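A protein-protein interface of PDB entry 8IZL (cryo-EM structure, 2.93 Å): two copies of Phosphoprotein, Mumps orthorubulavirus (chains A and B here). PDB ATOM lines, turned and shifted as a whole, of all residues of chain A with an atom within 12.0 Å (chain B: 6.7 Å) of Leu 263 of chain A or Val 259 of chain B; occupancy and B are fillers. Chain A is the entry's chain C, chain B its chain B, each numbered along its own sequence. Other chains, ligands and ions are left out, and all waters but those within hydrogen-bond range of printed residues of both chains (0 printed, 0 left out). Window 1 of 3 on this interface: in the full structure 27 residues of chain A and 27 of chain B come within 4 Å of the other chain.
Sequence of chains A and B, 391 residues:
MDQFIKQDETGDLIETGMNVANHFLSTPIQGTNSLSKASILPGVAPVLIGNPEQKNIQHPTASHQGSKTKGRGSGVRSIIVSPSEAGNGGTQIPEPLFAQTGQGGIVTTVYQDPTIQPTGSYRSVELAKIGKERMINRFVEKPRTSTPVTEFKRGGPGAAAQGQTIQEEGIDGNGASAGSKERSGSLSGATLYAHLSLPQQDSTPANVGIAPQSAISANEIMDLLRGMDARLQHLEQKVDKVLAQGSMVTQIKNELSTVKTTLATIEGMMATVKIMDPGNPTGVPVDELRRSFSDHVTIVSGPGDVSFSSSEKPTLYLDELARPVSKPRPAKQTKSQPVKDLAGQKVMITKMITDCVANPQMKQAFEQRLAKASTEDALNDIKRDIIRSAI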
ATOM      1  N   ILE A 252       3.082   4.551   9.335  1.00  0.00           N
ATOM      2  CA  ILE A 252       4.357   3.851   9.206  1.00  0.00           C
ATOM      3  C   ILE A 252       5.020   4.140   7.867  1.00  0.00           C
ATOM      4  O   ILE A 252       6.234   3.957   7.730  1.00  0.00           O
ATOM      5  CB  ILE A 252       4.172   2.334   9.416  1.00  0.00           C
ATOM      6  CG1 ILE A 252       3.409   1.693   8.252  1.00  0.00           C
ATOM      7  CG2 ILE A 252       3.454   2.063  10.727  1.00  0.00           C
ATOM      8  CD1 ILE A 252       4.290   0.987   7.233  1.00  0.00           C
ATOM      9  N   LYS A 253       4.251   4.584   6.868  1.00  0.00           N
ATOM     10  CA  LYS A 253       4.837   4.899   5.570  1.00  0.00           C
ATOM     11  C   LYS A 253       5.799   6.077   5.664  1.00  0.00           C
ATOM     12  O   LYS A 253       6.899   6.032   5.102  1.00  0.00           O
ATOM     13  CB  LYS A 253       3.730   5.180   4.553  1.00  0.00           C
ATOM     14  CG  LYS A 253       4.089   6.215   3.496  1.00  0.00           C
ATOM     15  CD  LYS A 253       4.946   5.613   2.394  1.00  0.00           C
ATOM     16  CE  LYS A 253       5.680   6.697   1.627  1.00  0.00           C
ATOM     17  NZ  LYS A 253       4.760   7.787   1.203  1.00  0.00           N
ATOM     18  N   ASN A 254       5.406   7.141   6.369  1.00  0.00           N
ATOM     19  CA  ASN A 254       6.282   8.303   6.481  1.00  0.00           C
ATOM     20  C   ASN A 254       7.435   8.039   7.442  1.00  0.00           C
ATOM     21  O   ASN A 254       8.568   8.462   7.189  1.00  0.00           O
ATOM     22  CB  ASN A 254       5.480   9.531   6.920  1.00  0.00           C
ATOM     23  CG  ASN A 254       4.537   9.233   8.066  1.00  0.00           C
ATOM     24  OD1 ASN A 254       3.374   8.886   7.854  1.00  0.00           O
ATOM     25  ND2 ASN A 254       5.029   9.370   9.292  1.00  0.00           N
ATOM     26  N   GLU A 255       7.165   7.342   8.549  1.00  0.00           N
ATOM     27  CA  GLU A 255       8.215   7.066   9.525  1.00  0.00           C
ATOM     28  C   GLU A 255       9.300   6.174   8.936  1.00  0.00           C
ATOM     29  O   GLU A 255      10.491   6.365   9.213  1.00  0.00           O
ATOM     30  CB  GLU A 255       7.619   6.427  10.778  1.00  0.00           C
ATOM     31  CG  GLU A 255       6.893   7.399  11.691  1.00  0.00           C
ATOM     32  CD  GLU A 255       5.498   6.929  12.046  1.00  0.00           C
ATOM     33  OE1 GLU A 255       5.252   5.706  11.998  1.00  0.00           O
ATOM     34  OE2 GLU A 255       4.646   7.784  12.372  1.00  0.00           O
ATOM     35  N   LEU A 256       8.909   5.186   8.126  1.00  0.00           N
ATOM     36  CA  LEU A 256       9.895   4.310   7.506  1.00  0.00           C
ATOM     37  C   LEU A 256      10.784   5.091   6.545  1.00  0.00           C
ATOM     38  O   LEU A 256      11.973   4.775   6.403  1.00  0.00           O
ATOM     39  CB  LEU A 256       9.179   3.149   6.805  1.00  0.00           C
ATOM     40  CG  LEU A 256       9.877   1.951   6.141  1.00  0.00           C
ATOM     41  CD1 LEU A 256      10.685   2.293   4.896  1.00  0.00           C
ATOM     42  CD2 LEU A 256      10.752   1.239   7.162  1.00  0.00           C
ATOM     43  N   SER A 257      10.234   6.117   5.891  1.00  0.00           N
ATOM     44  CA  SER A 257      11.049   6.965   5.026  1.00  0.00           C
ATOM     45  C   SER A 257      12.100   7.722   5.827  1.00  0.00           C
ATOM     46  O   SER A 257      13.211   7.955   5.341  1.00  0.00           O
ATOM     47  CB  SER A 257      10.159   7.935   4.249  1.00  0.00           C
ATOM     48  OG  SER A 257      10.881   8.558   3.200  1.00  0.00           O
ATOM     49  N   THR A 258      11.760   8.126   7.054  1.00  0.00           N
ATOM     50  CA  THR A 258      12.760   8.727   7.930  1.00  0.00           C
ATOM     51  C   THR A 258      13.874   7.737   8.244  1.00  0.00           C
ATOM     52  O   THR A 258      15.053   8.104   8.258  1.00  0.00           O
ATOM     53  CB  THR A 258      12.107   9.222   9.221  1.00  0.00           C
ATOM     54  OG1 THR A 258      11.822   8.104  10.072  1.00  0.00           O
ATOM     55  CG2 THR A 258      10.818   9.968   8.917  1.00  0.00           C
ATOM     56  N   VAL A 259      13.512   6.474   8.491  1.00  0.00           N
ATOM     57  CA  VAL A 259      14.512   5.444   8.756  1.00  0.00           C
ATOM     58  C   VAL A 259      15.411   5.246   7.543  1.00  0.00           C
ATOM     59  O   VAL A 259      16.635   5.123   7.671  1.00  0.00           O
ATOM     60  CB  VAL A 259      13.827   4.131   9.175  1.00  0.00           C
ATOM     61  CG1 VAL A 259      14.862   3.048   9.431  1.00  0.00           C
ATOM     62  CG2 VAL A 259      12.969   4.356  10.412  1.00  0.00           C
ATOM     63  N   LYS A 260      14.802   5.137   6.376  1.00  0.00           N
ATOM     64  CA  LYS A 260      15.586   4.887   5.185  1.00  0.00           C
ATOM     65  C   LYS A 260      16.709   5.899   5.100  1.00  0.00           C
ATOM     66  O   LYS A 260      17.864   5.535   4.887  1.00  0.00           O
ATOM     67  CB  LYS A 260      14.701   4.954   3.946  1.00  0.00           C
ATOM     68  CG  LYS A 260      15.467   5.121   2.649  1.00  0.00           C
ATOM     69  CD  LYS A 260      15.065   6.410   1.957  1.00  0.00           C
ATOM     70  CE  LYS A 260      13.608   6.739   2.229  1.00  0.00           C
ATOM     71  NZ  LYS A 260      13.421   8.177   2.548  1.00  0.00           N
ATOM     72  N   THR A 261      16.378   7.172   5.273  1.00  0.00           N
ATOM     73  CA  THR A 261      17.390   8.213   5.131  1.00  0.00           C
ATOM     74  C   THR A 261      18.536   8.142   6.143  1.00  0.00           C
ATOM     75  O   THR A 261      19.690   8.329   5.771  1.00  0.00           O
ATOM     76  CB  THR A 261      16.751   9.605   5.259  1.00  0.00           C
ATOM     77  OG1 THR A 261      16.197   9.759   6.569  1.00  0.00           O
ATOM     78  CG2 THR A 261      15.654   9.776   4.230  1.00  0.00           C
ATOM     79  N   THR A 262      18.230   7.863   7.405  1.00  0.00           N
ATOM     80  CA  THR A 262      19.298   7.731   8.398  1.00  0.00           C
ATOM     81  C   THR A 262      20.206   6.557   8.056  1.00  0.00           C
ATOM     82  O   THR A 262      21.423   6.649   8.189  1.00  0.00           O
ATOM     83  CB  THR A 262      18.786   7.602   9.853  1.00  0.00           C
ATOM     84  OG1 THR A 262      19.643   6.717  10.586  1.00  0.00           O
ATOM     85  CG2 THR A 262      17.375   7.071   9.890  1.00  0.00           C
ATOM     86  N   LEU A 263      19.611   5.457   7.611  1.00  0.00           N
ATOM     87  CA  LEU A 263      20.405   4.298   7.266  1.00  0.00           C
ATOM     88  C   LEU A 263      21.315   4.669   6.125  1.00  0.00           C
ATOM     89  O   LEU A 263      22.483   4.290   6.107  1.00  0.00           O
ATOM     90  CB  LEU A 263      19.507   3.141   6.844  1.00  0.00           C
ATOM     91  CG  LEU A 263      19.904   1.738   7.309  1.00  0.00           C
ATOM     92  CD1 LEU A 263      18.812   0.735   6.971  1.00  0.00           C
ATOM     93  CD2 LEU A 263      21.230   1.310   6.702  1.00  0.00           C
ATOM     94  N   ALA A 264      20.819   5.464   5.192  1.00  0.00           N
ATOM     95  CA  ALA A 264      21.694   5.931   4.136  1.00  0.00           C
ATOM     96  C   ALA A 264      22.814   6.752   4.752  1.00  0.00           C
ATOM     97  O   ALA A 264      23.983   6.565   4.416  1.00  0.00           O
ATOM     98  CB  ALA A 264      20.915   6.756   3.134  1.00  0.00           C
ATOM     99  N   THR A 265      22.466   7.658   5.657  1.00  0.00           N
ATOM    100  CA  THR A 265      23.468   8.536   6.259  1.00  0.00           C
ATOM    101  C   THR A 265      24.528   7.802   7.066  1.00  0.00           C
ATOM    102  O   THR A 265      25.713   8.123   6.976  1.00  0.00           O
ATOM    103  CB  THR A 265      22.806   9.564   7.189  1.00  0.00           C
ATOM    104  OG1 THR A 265      21.585  10.027   6.600  1.00  0.00           O
ATOM    105  CG2 THR A 265      23.736  10.743   7.417  1.00  0.00           C
ATOM    106  N   ILE A 266      24.115   6.802   7.834  1.00  0.00           N
ATOM    107  CA  ILE A 266      25.075   6.031   8.613  1.00  0.00           C
ATOM    108  C   ILE A 266      26.013   5.342   7.641  1.00  0.00           C
ATOM    109  O   ILE A 266      27.213   5.256   7.873  1.00  0.00           O
ATOM    110  CB  ILE A 266      24.423   5.025   9.588  1.00  0.00           C
ATOM    111  CG1 ILE A 266      23.649   5.771  10.676  1.00  0.00           C
ATOM    112  CG2 ILE A 266      25.451   4.109  10.219  1.00  0.00           C
ATOM    113  CD1 ILE A 266      22.765   4.878  11.516  1.00  0.00           C
ATOM    114  N   GLU A 267      25.463   4.856   6.540  1.00  0.00           N
ATOM    115  CA  GLU A 267      26.286   4.167   5.574  1.00  0.00           C
ATOM    116  C   GLU A 267      27.326   5.112   5.026  1.00  0.00           C
ATOM    117  O   GLU A 267      28.481   4.730   4.852  1.00  0.00           O
ATOM    118  CB  GLU A 267      25.424   3.643   4.435  1.00  0.00           C
ATOM    119  CG  GLU A 267      26.162   2.785   3.431  1.00  0.00           C
ATOM    120  CD  GLU A 267      25.217   1.940   2.612  1.00  0.00           C
ATOM    121  OE1 GLU A 267      24.440   1.174   3.218  1.00  0.00           O
ATOM    122  OE2 GLU A 267      25.247   2.038   1.367  1.00  0.00           O
ATOM    123  N   GLY A 268      26.923   6.349   4.771  1.00  0.00           N
ATOM    124  CA  GLY A 268      27.857   7.333   4.273  1.00  0.00           C
ATOM    125  C   GLY A 268      29.050   7.443   5.194  1.00  0.00           C
ATOM    126  O   GLY A 268      30.188   7.288   4.757  1.00  0.00           O
ATOM    127  N   MET A 269      28.797   7.697   6.472  1.00  0.00           N
ATOM    128  CA  MET A 269      29.889   7.872   7.424  1.00  0.00           C
ATOM    129  C   MET A 269      30.703   6.594   7.576  1.00  0.00           C
ATOM    130  O   MET A 269      31.928   6.645   7.643  1.00  0.00           O
ATOM    131  CB  MET A 269      29.354   8.343   8.779  1.00  0.00           C
ATOM    132  CG  MET A 269      28.387   7.385   9.448  1.00  0.00           C
ATOM    133  SD  MET A 269      27.451   8.172  10.771  1.00  0.00           S
ATOM    134  CE  MET A 269      26.547   9.412   9.845  1.00  0.00           C
ATOM    135  N   MET A 270      30.031   5.450   7.593  1.00  0.00           N
ATOM    136  CA  MET A 270      30.726   4.178   7.723  1.00  0.00           C
ATOM    137  C   MET A 270      31.619   3.930   6.524  1.00  0.00           C
ATOM    138  O   MET A 270      32.679   3.325   6.648  1.00  0.00           O
ATOM    139  CB  MET A 270      29.726   3.037   7.875  1.00  0.00           C
ATOM    140  CG  MET A 270      30.360   1.684   8.145  1.00  0.00           C
ATOM    141  SD  MET A 270      29.116   0.462   8.591  1.00  0.00           S
ATOM    142  CE  MET A 270      28.313   1.307   9.953  1.00  0.00           C
ATOM    143  N   ALA A 271      31.198   4.408   5.363  1.00  0.00           N
ATOM    144  CA  ALA A 271      31.985   4.220   4.157  1.00  0.00           C
ATOM    145  C   ALA A 271      33.219   5.108   4.165  1.00  0.00           C
ATOM    146  O   ALA A 271      34.168   4.856   3.431  1.00  0.00           O
ATOM    147  CB  ALA A 271      31.137   4.504   2.931  1.00  0.00           C
ATOM    148  N   THR A 272      33.214   6.142   4.996  1.00  0.00           N
ATOM    149  CA  THR A 272      34.341   7.072   5.039  1.00  0.00           C
ATOM    150  C   THR A 272      35.115   7.000   6.354  1.00  0.00           C
ATOM    151  O   THR A 272      35.773   7.962   6.745  1.00  0.00           O
ATOM    152  CB  THR A 272      33.875   8.521   4.799  1.00  0.00           C
ATOM    153  OG1 THR A 272      35.008   9.398   4.780  1.00  0.00           O
ATOM    154  CG2 THR A 272      32.917   8.965   5.890  1.00  0.00           C
ATOM    155  N   VAL A 273      35.056   5.859   7.031  1.00  0.00           N
ATOM    156  CA  VAL A 273      35.789   5.702   8.279  1.00  0.00           C
ATOM    157  C   VAL A 273      37.275   5.501   8.026  1.00  0.00           C
ATOM    158  O   VAL A 273      37.692   5.289   6.889  1.00  0.00           O
ATOM    159  CB  VAL A 273      35.256   4.521   9.103  1.00  0.00           C
ATOM    160  CG1 VAL A 273      33.825   4.783   9.543  1.00  0.00           C
ATOM    161  CG2 VAL A 273      35.350   3.230   8.305  1.00  0.00           C
ATOM    162  N   ASN B 254       8.722  -1.731  -2.099  1.00  0.00           N
ATOM    163  CA  ASN B 254       9.818  -1.302  -2.960  1.00  0.00           C
ATOM    164  C   ASN B 254      10.859  -0.516  -2.174  1.00  0.00           C
ATOM    165  O   ASN B 254      12.066  -0.676  -2.391  1.00  0.00           O
ATOM    166  CB  ASN B 254       9.276  -0.467  -4.119  1.00  0.00           C
ATOM    167  CG  ASN B 254      10.239  -0.389  -5.285  1.00  0.00           C
ATOM    168  OD1 ASN B 254      11.363  -0.888  -5.212  1.00  0.00           O
ATOM    169  ND2 ASN B 254       9.807   0.243  -6.370  1.00  0.00           N
ATOM    170  N   GLU B 255      10.413   0.341  -1.252  1.00  0.00           N
ATOM    171  CA  GLU B 255      11.356   1.117  -0.454  1.00  0.00           C
ATOM    172  C   GLU B 255      12.044   0.265   0.608  1.00  0.00           C
ATOM    173  O   GLU B 255      13.223   0.486   0.918  1.00  0.00           O
ATOM    174  CB  GLU B 255      10.634   2.308   0.178  1.00  0.00           C
ATOM    175  CG  GLU B 255      11.390   2.982   1.299  1.00  0.00           C
ATOM    176  CD  GLU B 255      10.599   4.104   1.927  1.00  0.00           C
ATOM    177  OE1 GLU B 255       9.463   4.359   1.472  1.00  0.00           O
ATOM    178  OE2 GLU B 255      11.115   4.736   2.866  1.00  0.00           O
ATOM    179  N   LEU B 256      11.344  -0.725   1.167  1.00  0.00           N
ATOM    180  CA  LEU B 256      11.995  -1.638   2.092  1.00  0.00           C
ATOM    181  C   LEU B 256      13.004  -2.529   1.389  1.00  0.00           C
ATOM    182  O   LEU B 256      13.903  -3.051   2.047  1.00  0.00           O
ATOM    183  CB  LEU B 256      10.965  -2.494   2.827  1.00  0.00           C
ATOM    184  CG  LEU B 256      11.473  -2.992   4.182  1.00  0.00           C
ATOM    185  CD1 LEU B 256      11.778  -1.809   5.083  1.00  0.00           C
ATOM    186  CD2 LEU B 256      10.489  -3.935   4.849  1.00  0.00           C
ATOM    187  N   SER B 257      12.886  -2.716   0.075  1.00  0.00           N
ATOM    188  CA  SER B 257      13.962  -3.375  -0.664  1.00  0.00           C
ATOM    189  C   SER B 257      15.255  -2.563  -0.587  1.00  0.00           C
ATOM    190  O   SER B 257      16.343  -3.112  -0.360  1.00  0.00           O
ATOM    191  CB  SER B 257      13.543  -3.591  -2.118  1.00  0.00           C
ATOM    192  OG  SER B 257      14.566  -4.239  -2.852  1.00  0.00           O
ATOM    193  N   THR B 258      15.149  -1.244  -0.766  1.00  0.00           N
ATOM    194  CA  THR B 258      16.313  -0.377  -0.614  1.00  0.00           C
ATOM    195  C   THR B 258      16.817  -0.393   0.824  1.00  0.00           C
ATOM    196  O   THR B 258      18.030  -0.374   1.071  1.00  0.00           O
ATOM    197  CB  THR B 258      15.964   1.047  -1.058  1.00  0.00           C
ATOM    198  OG1 THR B 258      15.973   1.115  -2.489  1.00  0.00           O
ATOM    199  CG2 THR B 258      16.966   2.053  -0.509  1.00  0.00           C
ATOM    200  N   VAL B 259      15.895  -0.432   1.786  1.00  0.00           N
ATOM    201  CA  VAL B 259      16.297  -0.560   3.185  1.00  0.00           C
ATOM    202  C   VAL B 259      17.078  -1.853   3.396  1.00  0.00           C
ATOM    203  O   VAL B 259      18.108  -1.870   4.084  1.00  0.00           O
ATOM    204  CB  VAL B 259      15.066  -0.477   4.105  1.00  0.00           C
ATOM    205  CG1 VAL B 259      15.368  -1.101   5.458  1.00  0.00           C
ATOM    206  CG2 VAL B 259      14.631   0.967   4.273  1.00  0.00           C
ATOM    207  N   LYS B 260      16.606  -2.951   2.802  1.00  0.00           N
ATOM    208  CA  LYS B 260      17.314  -4.227   2.873  1.00  0.00           C
ATOM    209  C   LYS B 260      18.735  -4.104   2.346  1.00  0.00           C
ATOM    210  O   LYS B 260      19.692  -4.523   3.005  1.00  0.00           O
ATOM    211  CB  LYS B 260      16.554  -5.294   2.083  1.00  0.00           C
ATOM    212  CG  LYS B 260      15.248  -5.778   2.691  1.00  0.00           C
ATOM    213  CD  LYS B 260      15.473  -6.953   3.632  1.00  0.00           C
ATOM    214  CE  LYS B 260      15.688  -6.513   5.062  1.00  0.00           C
ATOM    215  NZ  LYS B 260      15.979  -7.662   5.963  1.00  0.00           N
ATOM    216  N   THR B 261      18.893  -3.540   1.145  1.00  0.00           N
ATOM    217  CA  THR B 261      20.228  -3.525   0.551  1.00  0.00           C
ATOM    218  C   THR B 261      21.172  -2.604   1.322  1.00  0.00           C
ATOM    219  O   THR B 261      22.348  -2.945   1.522  1.00  0.00           O
ATOM    220  CB  THR B 261      20.176  -3.148  -0.934  1.00  0.00           C
ATOM    221  OG1 THR B 261      21.510  -3.055  -1.447  1.00  0.00           O
ATOM    222  CG2 THR B 261      19.484  -1.831  -1.155  1.00  0.00           C
ATOM    223  N   THR B 262      20.687  -1.453   1.797  1.00  0.00           N
ATOM    224  CA  THR B 262      21.579  -0.567   2.542  1.00  0.00           C
ATOM    225  C   THR B 262      21.921  -1.146   3.913  1.00  0.00           C
ATOM    226  O   THR B 262      23.056  -1.003   4.387  1.00  0.00           O
ATOM    227  CB  THR B 262      20.975   0.835   2.669  1.00  0.00           C
ATOM    228  OG1 THR B 262      21.910   1.697   3.327  1.00  0.00           O
ATOM    229  CG2 THR B 262      19.685   0.817   3.458  1.00  0.00           C
ATOM    230  N   LEU B 263      20.966  -1.829   4.555  1.00  0.00           N
ATOM    231  CA  LEU B 263      21.258  -2.484   5.823  1.00  0.00           C
ATOM    232  C   LEU B 263      22.269  -3.608   5.641  1.00  0.00           C
ATOM    233  O   LEU B 263      23.151  -3.802   6.484  1.00  0.00           O
ATOM    234  CB  LEU B 263      19.966  -3.015   6.443  1.00  0.00           C
ATOM    235  CG  LEU B 263      20.117  -4.032   7.574  1.00  0.00           C
ATOM    236  CD1 LEU B 263      20.686  -3.366   8.817  1.00  0.00           C
ATOM    237  CD2 LEU B 263      18.783  -4.696   7.874  1.00  0.00           C
ATOM    238  N   ALA B 264      22.158  -4.360   4.542  1.00  0.00           N
ATOM    239  CA  ALA B 264      23.144  -5.396   4.257  1.00  0.00           C
ATOM    240  C   ALA B 264      24.518  -4.793   4.013  1.00  0.00           C
ATOM    241  O   ALA B 264      25.536  -5.356   4.438  1.00  0.00           O
ATOM    242  CB  ALA B 264      22.700  -6.227   3.054  1.00  0.00           C
ATOM    243  N   ILE B 266      25.657  -2.015   5.349  1.00  0.00           N
ATOM    244  CA  ILE B 266      26.158  -1.622   6.666  1.00  0.00           C
ATOM    245  C   ILE B 266      26.654  -2.840   7.434  1.00  0.00           C
ATOM    246  O   ILE B 266      27.711  -2.799   8.081  1.00  0.00           O
ATOM    247  CB  ILE B 266      25.064  -0.867   7.447  1.00  0.00           C
ATOM    248  CG1 ILE B 266      24.704   0.439   6.740  1.00  0.00           C
ATOM    249  CG2 ILE B 266      25.515  -0.608   8.877  1.00  0.00           C
ATOM    250  CD1 ILE B 266      25.475   1.641   7.231  1.00  0.00           C
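Ser 257 of chain A touches Glu 255 of chain B, but with the chains exchanged Glu 255 of chain A does not touch Ser 257 of chain B (13.1 Å). Leu 263 of chain A touches Val 259 of chain B, but with the chains exchanged Val 259 of chain A does not touch Leu 263 of chain B (8.5 Å). Leu 263 of chain A touches Thr 262 of chain B, but with the chains exchanged Thr 262 of chain A does not touch Leu 263 of chain B (9.1 Å). Leu 263 of chain B touches its own counterpart, Leu 263 of chain A. Positions printed for both chains: 254, 255, 256, 257, 258, 259, 260, 261, 262, 263, 264 and 266.
Printed residues of chain A that touch a printed residue of chain B: Leu 256, Ser 257, Lys 260, Leu 263, Ile 266, Glu 267 and Met 270. Among the printed residues, 12 pairs touch across the chains.
The side-chain carboxylate (OE2) of Glu 255 of chain B sits close to the backbone NH (N) of Ser 257 of chain A. OE1 of Glu 267 of chain A is in hydrogen-bond range of OG1 of Thr 262 of chain B (2.6 Å). SD of Met 270 of chain A lies close to O of Ile 266 of chain B, at 3.6 Å.
Printed residues of chain B within 4 Å of Leu 263 of chain A: Val 259, Thr 262, Leu 263 and Ile 266. Printed residues of chain A within 4 Å of Val 259 of chain B: Leu 263. Of chain A, only Leu 256, Ser 257 and Lys 260 come within 4 Å of Glu 255 of chain B. Leu 256 of chain B touches just one residue of chain A: Leu 256. No residue of chain A comes within 4 Å of Ser 257 of chain B. No residue of chain A comes within 4 Å of Thr 258 of chain B. Lys 260 of chain B touches none of the printed residues of chain A. No residue of chain A comes within 4 Å of Thr 261 of chain B. Of chain A, only Leu 263 and Glu 267 come within 4 Å of Thr 262 of chain B. Leu 263 of chain B touches one residue of chain A. Of chain A, only Leu 263 (3.6 Å), Ile 266 (3.8 Å), Glu 267 (3.1 Å) and Met 270 (3.6 Å) come within 4 Å of Ile 266 of chain B. Of the printed residues of chain B, Met 270 of chain A touches Ile 266 (3.6 Å). Of the printed residues of chain B, Ile 266 of chain A touches Ile 266 (3.8 Å). Printed residues of chain B within 4 Å of Ser 257 of chain A: Glu 255 (3.1 Å). Printed residues of chain B within 4 Å of Lys 260 of chain A: Glu 255. Printed residues of chain B within 4 Å of Leu 256 of chain A: Glu 255 (3.2 Å) and Leu 256 (3.8 Å). The nearest residue of chain B that does not touch Leu 263 of chain A is Lys 260 of chain B (6.0 Å).
The side-chain hydroxyl (OG) of Ser 257 of chain A sits at hydrogen-bond distance from the side-chain amino group (NZ) of Lys 260 of chain A (2.6 Å).
CD1 of Leu 256 of chain A touches OE2 of Glu 255 of chain B, at 3.2 Å. CD2 of Leu 256 of chain A touches CD1 of Leu 256 of chain B, at 3.8 Å. Lys 260 of chain A touches Glu 255 of chain B. CD1 of Leu 263 of chain A touches O of Val 259 of chain B (3.95 Å). OG1 of Thr 262 of chain B touches CD2 of Leu 263 of chain A, 3.5 Å away. Leu 263 of chain B touches Leu 263 of chain A (N to CD2, 3.8 Å). Leu 263 of chain A touches Ile 266 of chain B (CD2 to CG1, 3.6 Å). CD1 of Ile 266 of chain B touches C of Ile 266 of chain A, at 3.8 Å. CD1 of Ile 266 of chain B touches CA of Glu 267 of chain A (3.1 Å).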
